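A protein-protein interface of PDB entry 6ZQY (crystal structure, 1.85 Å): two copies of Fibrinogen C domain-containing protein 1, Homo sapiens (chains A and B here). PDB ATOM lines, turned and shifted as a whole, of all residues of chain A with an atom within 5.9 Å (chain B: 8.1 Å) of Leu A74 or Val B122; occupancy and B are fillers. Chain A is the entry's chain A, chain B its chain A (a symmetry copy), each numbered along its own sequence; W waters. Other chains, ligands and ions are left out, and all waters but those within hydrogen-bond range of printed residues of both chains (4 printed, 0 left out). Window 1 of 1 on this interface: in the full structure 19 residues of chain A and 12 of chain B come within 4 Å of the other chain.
The backbone carbonyl oxygen of Leu B119 sits close to the side-chain amide oxygen of Gln A35 (3.3 Å). The backbone carbonyl oxygen (O) of Gly A72 is in hydrogen-bond range of the backbone NH (N) of Val B122 (3.1 Å). The side-chain carboxylate (OD2) of Asp B127 lies within salt-bridge range of the guanidinium group (NE) of Arg A73, at 2.7 Å. The backbone carbonyl oxygen of Phe B120 lies within hydrogen-bond range of the backbone NH of Leu A74, 2.9 Å away. The guanidinium group (NH2) of Arg A84 lies within hydrogen-bond range of the backbone carbonyl oxygen (O) of Val B122 (3.5 Å).
The backbone carbonyl oxygen (O) of His A78 lies within hydrogen-bond range of the backbone NH (N) of Arg A52 (3.0 Å). O of Arg A73 is in hydrogen-bond range of ND1 of His A78 (3.2 Å). A ring nitrogen (ND1) of His A78 sits at hydrogen-bond distance from the backbone carbonyl oxygen (O) of Gly A76, at 2.9 Å. The side-chain carboxylate (OD2) of Asp B127 lies within hydrogen-bond range of the side-chain hydroxyl (OG) of Ser B121, at 2.6 Å. N of Glu B125 sits close to OD1 of Asp B123. OD1 of Asp B123 lies within hydrogen-bond range of N of Glu B126 (3.3 Å).
CG2 of Val A22 touches CD1 of Phe B120, 3.8 Å away. Val B122 touches Gly A70 (CG1 to CA, 3.7 Å). O of Gly A70 touches CB of Asp B123, at 3.5 Å. Val B122 touches Phe A71. CA of Phe A71 touches OE2 of Glu B126 (3.6 Å). Gly A72 touches Ser B121 (O to CA, 3.9 Å). N of Gly A72 touches OE2 of Glu B126, 3.6 Å away. Phe B120 touches Arg A73. Leu A74 touches Val B122 (CD2 to CG2, 3.8 Å). Thr A75 touches Phe B120 (CG2 to CD1, 3.7 Å).
Of the printed residues of chain B, Val A22 touches Phe B120 (3.8 Å). Of chain B, only Phe B120 and Val B122 come within 4 Å of Leu A74. Of the printed residues of chain B, Arg A84 touches Val B122. Of the printed residues of chain A, Phe B120 touches Val A22, Arg A73, Leu A74 and Thr A75. Val B122 touches eight residues of chain A. Printed residues of chain A within 4 Å of Asp B127: Arg A73. The nearest residue of chain B that does not touch Leu A74 is Ser B121 (5.1 Å). The nearest printed residue of chain B that does not touch Leu A80 is Asp B123 (6.5 Å).
Of the 11 printed residues of chain B, 7 touch a printed residue of chain A. Printed residues of chain B that touch a printed residue of chain A: Leu B119, Phe B120, Ser B121, Val B122, Asp B123, Glu B126 and Asp B127. Hydrophobic or aromatic side chains of chain B that line the printed part of chain A: Phe B120 and Val B122. Along chain B the printed residues that touch a printed residue of chain A span positions 119 to 127. Hydrophobic or aromatic side chains of chain A within 4 Å of the printed part of chain B: Val A22, Phe A71, Leu A74 and His A78. Among the printed residues, 19 pairs touch across the chains.
No position is printed for both chains.
Water W2 lies within hydrogen-bond range of the backbone carbonyl oxygen (O) of Gly A70 (2.6 Å) and the side-chain carboxylate (OD2) of Asp B123 (2.7 Å). Water W4 lies within hydrogen-bond range of the side-chain carboxylate of Glu B126, the backbone carbonyl oxygen of Gly A72, the backbone NH of Asp B123 and the backbone NH of Val B122. Water W1 lies within hydrogen-bond range of O of Val B122 and NH2 of Arg A84. Water W3 lies within hydrogen-bond range of the backbone NH (N) of Gly A72 (3.2 Å) and the side-chain carboxylate (OE2) of Glu B126 (3.2 Å).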
ATOM      1  N   VAL A  22      15.260  24.240   6.793  1.00  0.00           N
ATOM      2  CA  VAL A  22      16.510  24.749   7.422  1.00  0.00           C
ATOM      3  C   VAL A  22      16.132  25.518   8.687  1.00  0.00           C
ATOM      4  O   VAL A  22      15.215  26.365   8.617  1.00  0.00           O
ATOM      5  CB  VAL A  22      17.315  25.611   6.435  1.00  0.00           C
ATOM      6  CG1 VAL A  22      18.519  26.263   7.096  1.00  0.00           C
ATOM      7  CG2 VAL A  22      17.737  24.798   5.220  1.00  0.00           C
ATOM      8  N   GLN A  35      23.107  26.658  11.077  1.00  0.00           N
ATOM      9  CA  GLN A  35      21.886  26.190  10.380  1.00  0.00           C
ATOM     10  C   GLN A  35      22.089  24.725   9.986  1.00  0.00           C
ATOM     11  O   GLN A  35      23.243  24.322   9.690  1.00  0.00           O
ATOM     12  CB  GLN A  35      21.560  27.123   9.215  1.00  0.00           C
ATOM     13  CG  GLN A  35      21.099  28.501   9.672  1.00  0.00           C
ATOM     14  CD  GLN A  35      20.650  29.365   8.520  1.00  0.00           C
ATOM     15  OE1 GLN A  35      21.227  29.341   7.440  1.00  0.00           O
ATOM     16  NE2 GLN A  35      19.603  30.137   8.738  1.00  0.00           N
ATOM     17  N   VAL A  36      21.002  23.956  10.022  1.00  0.00           N
ATOM     18  CA  VAL A  36      20.961  22.517   9.648  1.00  0.00           C
ATOM     19  C   VAL A  36      19.668  22.257   8.878  1.00  0.00           C
ATOM     20  O   VAL A  36      18.723  23.048   9.021  1.00  0.00           O
ATOM     21  CB  VAL A  36      21.024  21.605  10.885  1.00  0.00           C
ATOM     22  CG1 VAL A  36      22.359  21.722  11.601  1.00  0.00           C
ATOM     23  CG2 VAL A  36      19.865  21.871  11.844  1.00  0.00           C
ATOM     24  N   TYR A  37      19.614  21.148   8.151  1.00  0.00           N
ATOM     25  CA  TYR A  37      18.349  20.622   7.589  1.00  0.00           C
ATOM     26  C   TYR A  37      17.728  19.658   8.602  1.00  0.00           C
ATOM     27  O   TYR A  37      18.415  18.727   9.061  1.00  0.00           O
ATOM     28  CB  TYR A  37      18.562  19.971   6.223  1.00  0.00           C
ATOM     29  CG  TYR A  37      17.268  19.856   5.461  1.00  0.00           C
ATOM     30  CD1 TYR A  37      16.346  18.868   5.766  1.00  0.00           C
ATOM     31  CD2 TYR A  37      16.934  20.781   4.488  1.00  0.00           C
ATOM     32  CE1 TYR A  37      15.142  18.774   5.085  1.00  0.00           C
ATOM     33  CE2 TYR A  37      15.736  20.702   3.798  1.00  0.00           C
ATOM     34  CZ  TYR A  37      14.838  19.696   4.099  1.00  0.00           C
ATOM     35  OH  TYR A  37      13.652  19.629   3.428  1.00  0.00           O
ATOM     36  N   ARG A  52      24.060  14.296   2.861  1.00  0.00           N
ATOM     37  CA  ARG A  52      23.066  14.002   1.800  1.00  0.00           C
ATOM     38  C   ARG A  52      23.772  13.866   0.448  1.00  0.00           C
ATOM     39  O   ARG A  52      24.542  14.768   0.081  1.00  0.00           O
ATOM     40  CB  ARG A  52      21.983  15.077   1.712  1.00  0.00           C
ATOM     41  CG  ARG A  52      20.871  14.698   0.739  1.00  0.00           C
ATOM     42  CD  ARG A  52      19.835  15.784   0.548  1.00  0.00           C
ATOM     43  NE  ARG A  52      19.075  16.020   1.763  1.00  0.00           N
ATOM     44  CZ  ARG A  52      18.952  17.188   2.383  1.00  0.00           C
ATOM     45  NH1 ARG A  52      19.538  18.281   1.911  1.00  0.00           N
ATOM     46  NH2 ARG A  52      18.222  17.260   3.482  1.00  0.00           N
ATOM     47  N   ASP A  69      35.076  21.281   8.408  1.00  0.00           N
ATOM     48  CA  ASP A  69      34.338  22.574   8.406  1.00  0.00           C
ATOM     49  C   ASP A  69      33.005  22.441   7.666  1.00  0.00           C
ATOM     50  O   ASP A  69      32.129  23.287   7.901  1.00  0.00           O
ATOM     51  CB  ASP A  69      35.194  23.690   7.806  1.00  0.00           C
ATOM     52  CG  ASP A  69      36.406  24.028   8.654  1.00  0.00           C
ATOM     53  OD1 ASP A  69      36.372  23.745   9.863  1.00  0.00           O
ATOM     54  OD2 ASP A  69      37.384  24.535   8.090  1.00  0.00           O
ATOM     55  N   GLY A  70      32.859  21.433   6.807  1.00  0.00           N
ATOM     56  CA  GLY A  70      31.616  21.180   6.052  1.00  0.00           C
ATOM     57  C   GLY A  70      31.658  21.795   4.663  1.00  0.00           C
ATOM     58  O   GLY A  70      32.526  22.663   4.407  1.00  0.00           O
ATOM     59  N   PHE A  71      30.759  21.350   3.784  1.00  0.00           N
ATOM     60  CA  PHE A  71      30.670  21.806   2.373  1.00  0.00           C
ATOM     61  C   PHE A  71      29.307  21.434   1.790  1.00  0.00           C
ATOM     62  O   PHE A  71      28.546  20.669   2.425  1.00  0.00           O
ATOM     63  CB  PHE A  71      31.824  21.235   1.542  1.00  0.00           C
ATOM     64  CG  PHE A  71      31.924  19.730   1.536  1.00  0.00           C
ATOM     65  CD1 PHE A  71      31.254  18.976   0.584  1.00  0.00           C
ATOM     66  CD2 PHE A  71      32.696  19.066   2.479  1.00  0.00           C
ATOM     67  CE1 PHE A  71      31.349  17.593   0.580  1.00  0.00           C
ATOM     68  CE2 PHE A  71      32.796  17.681   2.468  1.00  0.00           C
ATOM     69  CZ  PHE A  71      32.122  16.948   1.521  1.00  0.00           C
ATOM     70  N   GLY A  72      29.015  21.988   0.612  1.00  0.00           N
ATOM     71  CA  GLY A  72      27.717  21.838  -0.064  1.00  0.00           C
ATOM     72  C   GLY A  72      26.678  22.759   0.541  1.00  0.00           C
ATOM     73  O   GLY A  72      27.063  23.709   1.276  1.00  0.00           O
ATOM     74  N   ARG A  73      25.404  22.492   0.251  1.00  0.00           N
ATOM     75  CA  ARG A  73      24.270  23.346   0.682  1.00  0.00           C
ATOM     76  C   ARG A  73      23.234  22.491   1.411  1.00  0.00           C
ATOM     77  O   ARG A  73      23.014  21.332   1.010  1.00  0.00           O
ATOM     78  CB  ARG A  73      23.693  24.097  -0.520  1.00  0.00           C
ATOM     79  CG  ARG A  73      24.656  25.144  -1.057  1.00  0.00           C
ATOM     80  CD  ARG A  73      24.206  25.849  -2.318  1.00  0.00           C
ATOM     81  NE  ARG A  73      25.309  26.627  -2.873  1.00  0.00           N
ATOM     82  CZ  ARG A  73      25.346  27.146  -4.099  1.00  0.00           C
ATOM     83  NH1 ARG A  73      24.328  26.980  -4.932  1.00  0.00           N
ATOM     84  NH2 ARG A  73      26.409  27.829  -4.494  1.00  0.00           N
ATOM     85  N   LEU A  74      22.628  23.068   2.445  1.00  0.00           N
ATOM     86  CA  LEU A  74      21.711  22.357   3.374  1.00  0.00           C
ATOM     87  C   LEU A  74      20.480  21.850   2.616  1.00  0.00           C
ATOM     88  O   LEU A  74      19.916  20.835   3.051  1.00  0.00           O
ATOM     89  CB  LEU A  74      21.310  23.314   4.500  1.00  0.00           C
ATOM     90  CG  LEU A  74      22.450  23.755   5.409  1.00  0.00           C
ATOM     91  CD1 LEU A  74      21.995  24.871   6.336  1.00  0.00           C
ATOM     92  CD2 LEU A  74      22.999  22.578   6.202  1.00  0.00           C
ATOM     93  N   THR A  75      20.093  22.536   1.538  1.00  0.00           N
ATOM     94  CA  THR A  75      18.905  22.227   0.699  1.00  0.00           C
ATOM     95  C   THR A  75      19.246  21.157  -0.350  1.00  0.00           C
ATOM     96  O   THR A  75      18.315  20.687  -1.035  1.00  0.00           O
ATOM     97  CB  THR A  75      18.369  23.515   0.061  1.00  0.00           C
ATOM     98  OG1 THR A  75      19.444  24.178  -0.606  1.00  0.00           O
ATOM     99  CG2 THR A  75      17.759  24.448   1.081  1.00  0.00           C
ATOM    100  N   GLY A  76      20.519  20.771  -0.475  1.00  0.00           N
ATOM    101  CA  GLY A  76      20.969  19.781  -1.472  1.00  0.00           C
ATOM    102  C   GLY A  76      21.992  18.820  -0.900  1.00  0.00           C
ATOM    103  O   GLY A  76      21.877  18.449   0.287  1.00  0.00           O
ATOM    104  N   GLU A  77      22.960  18.425  -1.723  1.00  0.00           N
ATOM    105  CA  GLU A  77      24.074  17.548  -1.306  1.00  0.00           C
ATOM    106  C   GLU A  77      24.967  18.348  -0.362  1.00  0.00           C
ATOM    107  O   GLU A  77      25.282  19.512  -0.681  1.00  0.00           O
ATOM    108  CB  GLU A  77      24.865  17.066  -2.517  1.00  0.00           C
ATOM    109  CG  GLU A  77      24.060  16.205  -3.462  1.00  0.00           C
ATOM    110  CD  GLU A  77      24.946  15.392  -4.381  1.00  0.00           C
ATOM    111  OE1 GLU A  77      25.983  15.938  -4.804  1.00  0.00           O
ATOM    112  OE2 GLU A  77      24.619  14.207  -4.639  1.00  0.00           O
ATOM    113  N   HIS A  78      25.325  17.770   0.779  1.00  0.00           N
ATOM    114  CA  HIS A  78      26.193  18.455   1.764  1.00  0.00           C
ATOM    115  C   HIS A  78      26.772  17.461   2.760  1.00  0.00           C
ATOM    116  O   HIS A  78      26.294  16.306   2.840  1.00  0.00           O
ATOM    117  CB  HIS A  78      25.438  19.593   2.463  1.00  0.00           C
ATOM    118  CG  HIS A  78      24.347  19.164   3.388  1.00  0.00           C
ATOM    119  ND1 HIS A  78      23.099  18.784   2.939  1.00  0.00           N
ATOM    120  CD2 HIS A  78      24.296  19.099   4.736  1.00  0.00           C
ATOM    121  CE1 HIS A  78      22.329  18.497   3.973  1.00  0.00           C
ATOM    122  NE2 HIS A  78      23.041  18.680   5.084  1.00  0.00           N
ATOM    123  N   TRP A  79      27.803  17.934   3.444  1.00  0.00           N
ATOM    124  CA  TRP A  79      28.429  17.337   4.642  1.00  0.00           C
ATOM    125  C   TRP A  79      28.476  18.443   5.693  1.00  0.00           C
ATOM    126  O   TRP A  79      29.078  19.491   5.397  1.00  0.00           O
ATOM    127  CB  TRP A  79      29.823  16.816   4.301  1.00  0.00           C
ATOM    128  CG  TRP A  79      30.552  16.289   5.493  1.00  0.00           C
ATOM    129  CD1 TRP A  79      31.500  16.928   6.237  1.00  0.00           C
ATOM    130  CD2 TRP A  79      30.389  14.986   6.071  1.00  0.00           C
ATOM    131  NE1 TRP A  79      31.918  16.122   7.259  1.00  0.00           N
ATOM    132  CE2 TRP A  79      31.265  14.916   7.173  1.00  0.00           C
ATOM    133  CE3 TRP A  79      29.583  13.880   5.771  1.00  0.00           C
ATOM    134  CZ2 TRP A  79      31.359  13.777   7.972  1.00  0.00           C
ATOM    135  CZ3 TRP A  79      29.691  12.750   6.550  1.00  0.00           C
ATOM    136  CH2 TRP A  79      30.563  12.704   7.640  1.00  0.00           C
ATOM    137  N   LEU A  80      27.843  18.247   6.846  1.00  0.00           N
ATOM    138  CA  LEU A  80      27.656  19.342   7.832  1.00  0.00           C
ATOM    139  C   LEU A  80      29.007  19.759   8.427  1.00  0.00           C
ATOM    140  O   LEU A  80      29.126  20.934   8.845  1.00  0.00           O
ATOM    141  CB  LEU A  80      26.688  18.876   8.920  1.00  0.00           C
ATOM    142  CG  LEU A  80      26.253  19.947   9.918  1.00  0.00           C
ATOM    143  CD1 LEU A  80      25.523  21.080   9.217  1.00  0.00           C
ATOM    144  CD2 LEU A  80      25.376  19.331  10.996  1.00  0.00           C
ATOM    145  N   GLY A  81      29.970  18.836   8.481  1.00  0.00           N
ATOM    146  CA  GLY A  81      31.304  19.077   9.055  1.00  0.00           C
ATOM    147  C   GLY A  81      31.466  18.363  10.384  1.00  0.00           C
ATOM    148  O   GLY A  81      30.554  18.444  11.235  1.00  0.00           O
ATOM    149  N   ARG A  84      30.887  20.226  13.706  1.00  0.00           N
ATOM    150  CA  ARG A  84      29.442  20.382  14.031  1.00  0.00           C
ATOM    151  C   ARG A  84      28.861  19.044  14.508  1.00  0.00           C
ATOM    152  O   ARG A  84      28.060  19.056  15.457  1.00  0.00           O
ATOM    153  CB  ARG A  84      28.683  20.946  12.829  1.00  0.00           C
ATOM    154  CG  ARG A  84      29.197  22.308  12.393  1.00  0.00           C
ATOM    155  CD  ARG A  84      28.217  23.043  11.513  1.00  0.00           C
ATOM    156  NE  ARG A  84      28.742  24.342  11.120  1.00  0.00           N
ATOM    157  CZ  ARG A  84      29.606  24.548  10.139  1.00  0.00           C
ATOM    158  NH1 ARG A  84      30.072  23.537   9.420  1.00  0.00           N
ATOM    159  NH2 ARG A  84      30.007  25.780   9.874  1.00  0.00           N
ATOM    160  N   HIS B  86      26.683  37.686   5.464  1.00  0.00           N
ATOM    161  CA  HIS B  86      26.121  36.319   5.651  1.00  0.00           C
ATOM    162  C   HIS B  86      25.382  36.221   6.999  1.00  0.00           C
ATOM    163  O   HIS B  86      24.239  35.721   6.999  1.00  0.00           O
ATOM    164  CB  HIS B  86      27.196  35.231   5.543  1.00  0.00           C
ATOM    165  CG  HIS B  86      26.677  33.892   5.951  1.00  0.00           C
ATOM    166  ND1 HIS B  86      26.825  33.396   7.237  1.00  0.00           N
ATOM    167  CD2 HIS B  86      25.952  32.979   5.276  1.00  0.00           C
ATOM    168  CE1 HIS B  86      26.235  32.217   7.321  1.00  0.00           C
ATOM    169  NE2 HIS B  86      25.686  31.943   6.134  1.00  0.00           N
ATOM    170  N   GLY B 118      25.212  33.492   0.679  1.00  0.00           N
ATOM    171  CA  GLY B 118      25.454  32.118   1.164  1.00  0.00           C
ATOM    172  C   GLY B 118      24.340  31.594   2.061  1.00  0.00           C
ATOM    173  O   GLY B 118      24.665  30.942   3.077  1.00  0.00           O
ATOM    174  N   LEU B 119      23.075  31.819   1.688  1.00  0.00           N
ATOM    175  CA  LEU B 119      21.899  31.609   2.583  1.00  0.00           C
ATOM    176  C   LEU B 119      21.795  30.154   3.064  1.00  0.00           C
ATOM    177  O   LEU B 119      21.275  29.954   4.188  1.00  0.00           O
ATOM    178  CB  LEU B 119      20.607  32.015   1.865  1.00  0.00           C
ATOM    179  CG  LEU B 119      20.347  33.516   1.739  1.00  0.00           C
ATOM    180  CD1 LEU B 119      18.947  33.760   1.188  1.00  0.00           C
ATOM    181  CD2 LEU B 119      20.523  34.231   3.073  1.00  0.00           C
ATOM    182  N   PHE B 120      22.214  29.180   2.253  1.00  0.00           N
ATOM    183  CA  PHE B 120      22.068  27.728   2.563  1.00  0.00           C
ATOM    184  C   PHE B 120      23.430  27.028   2.549  1.00  0.00           C
ATOM    185  O   PHE B 120      23.473  25.792   2.628  1.00  0.00           O
ATOM    186  CB  PHE B 120      21.093  27.083   1.578  1.00  0.00           C
ATOM    187  CG  PHE B 120      19.699  27.653   1.649  1.00  0.00           C
ATOM    188  CD1 PHE B 120      18.919  27.464   2.780  1.00  0.00           C
ATOM    189  CD2 PHE B 120      19.170  28.383   0.597  1.00  0.00           C
ATOM    190  CE1 PHE B 120      17.635  27.983   2.851  1.00  0.00           C
ATOM    191  CE2 PHE B 120      17.888  28.905   0.671  1.00  0.00           C
ATOM    192  CZ  PHE B 120      17.121  28.701   1.794  1.00  0.00           C
ATOM    193  N   SER B 121      24.512  27.799   2.465  1.00  0.00           N
ATOM    194  CA  SER B 121      25.903  27.294   2.377  1.00  0.00           C
ATOM    195  C   SER B 121      26.323  26.746   3.744  1.00  0.00           C
ATOM    196  O   SER B 121      26.211  27.491   4.727  1.00  0.00           O
ATOM    197  CB  SER B 121      26.825  28.386   1.901  1.00  0.00           C
ATOM    198  OG  SER B 121      26.373  28.914   0.661  1.00  0.00           O
ATOM    199  N   VAL B 122      26.753  25.486   3.812  1.00  0.00           N
ATOM    200  CA  VAL B 122      27.246  24.862   5.077  1.00  0.00           C
ATOM    201  C   VAL B 122      28.449  25.675   5.563  1.00  0.00           C
ATOM    202  O   VAL B 122      28.487  26.008   6.765  1.00  0.00           O
ATOM    203  CB  VAL B 122      27.620  23.382   4.890  1.00  0.00           C
ATOM    204  CG1 VAL B 122      28.343  22.838   6.110  1.00  0.00           C
ATOM    205  CG2 VAL B 122      26.404  22.533   4.566  1.00  0.00           C
ATOM    206  N   ASP B 123      29.397  25.940   4.658  1.00  0.00           N
ATOM    207  CA  ASP B 123      30.574  26.825   4.872  1.00  0.00           C
ATOM    208  C   ASP B 123      30.487  27.951   3.845  1.00  0.00           C
ATOM    209  O   ASP B 123      30.978  27.816   2.727  1.00  0.00           O
ATOM    210  CB  ASP B 123      31.881  26.034   4.803  1.00  0.00           C
ATOM    211  CG  ASP B 123      33.147  26.866   4.966  1.00  0.00           C
ATOM    212  OD1 ASP B 123      33.036  28.097   5.074  1.00  0.00           O
ATOM    213  OD2 ASP B 123      34.239  26.269   4.974  1.00  0.00           O
ATOM    214  N   PRO B 124      29.834  29.088   4.183  1.00  0.00           N
ATOM    215  CA  PRO B 124      29.632  30.165   3.214  1.00  0.00           C
ATOM    216  C   PRO B 124      30.939  30.642   2.565  1.00  0.00           C
ATOM    217  O   PRO B 124      30.896  30.984   1.405  1.00  0.00           O
ATOM    218  CB  PRO B 124      28.942  31.285   4.011  1.00  0.00           C
ATOM    219  CG  PRO B 124      29.120  30.911   5.473  1.00  0.00           C
ATOM    220  CD  PRO B 124      29.254  29.401   5.497  1.00  0.00           C
ATOM    221  N   GLU B 125      32.065  30.609   3.284  1.00  0.00           N
ATOM    222  CA  GLU B 125      33.374  31.037   2.719  1.00  0.00           C
ATOM    223  C   GLU B 125      33.815  30.064   1.620  1.00  0.00           C
ATOM    224  O   GLU B 125      34.215  30.544   0.545  1.00  0.00           O
ATOM    225  CB  GLU B 125      34.476  31.161   3.772  1.00  0.00           C
ATOM    226  CG  GLU B 125      35.761  31.709   3.168  1.00  0.00           C
ATOM    227  CD  GLU B 125      36.960  31.858   4.083  1.00  0.00           C
ATOM    228  OE1 GLU B 125      36.849  31.495   5.266  1.00  0.00           O
ATOM    229  OE2 GLU B 125      38.001  32.351   3.599  1.00  0.00           O
ATOM    230  N   GLU B 126      33.772  28.752   1.875  1.00  0.00           N
ATOM    231  CA  GLU B 126      34.235  27.738   0.887  1.00  0.00           C
ATOM    232  C   GLU B 126      33.284  27.778  -0.313  1.00  0.00           C
ATOM    233  O   GLU B 126      33.772  27.654  -1.457  1.00  0.00           O
ATOM    234  CB  GLU B 126      34.370  26.342   1.507  1.00  0.00           C
ATOM    235  CG  GLU B 126      33.072  25.556   1.629  1.00  0.00           C
ATOM    236  CD  GLU B 126      32.668  24.692   0.442  1.00  0.00           C
ATOM    237  OE1 GLU B 126      33.568  24.148  -0.232  1.00  0.00           O
ATOM    238  OE2 GLU B 126      31.452  24.558   0.197  1.00  0.00           O
ATOM    239  N   ASP B 127      31.993  28.004  -0.063  1.00  0.00           N
ATOM    240  CA  ASP B 127      30.934  28.025  -1.107  1.00  0.00           C
ATOM    241  C   ASP B 127      30.937  29.361  -1.869  1.00  0.00           C
ATOM    242  O   ASP B 127      30.147  29.481  -2.823  1.00  0.00           O
ATOM    243  CB  ASP B 127      29.562  27.738  -0.498  1.00  0.00           C
ATOM    244  CG  ASP B 127      28.536  27.258  -1.510  1.00  0.00           C
ATOM    245  OD1 ASP B 127      28.946  26.617  -2.499  1.00  0.00           O
ATOM    246  OD2 ASP B 127      27.344  27.538  -1.311  1.00  0.00           O
HETATM  247  O   HOH W   1      27.740  28.035   8.691  1.00  0.00           O
HETATM  248  O   HOH W   2      34.882  23.783   4.295  1.00  0.00           O
HETATM  249  O   HOH W   3      30.852  22.270  -2.005  1.00  0.00           O
HETATM  250  O   HOH W   4      29.364  25.198   1.818  1.00  0.00           O
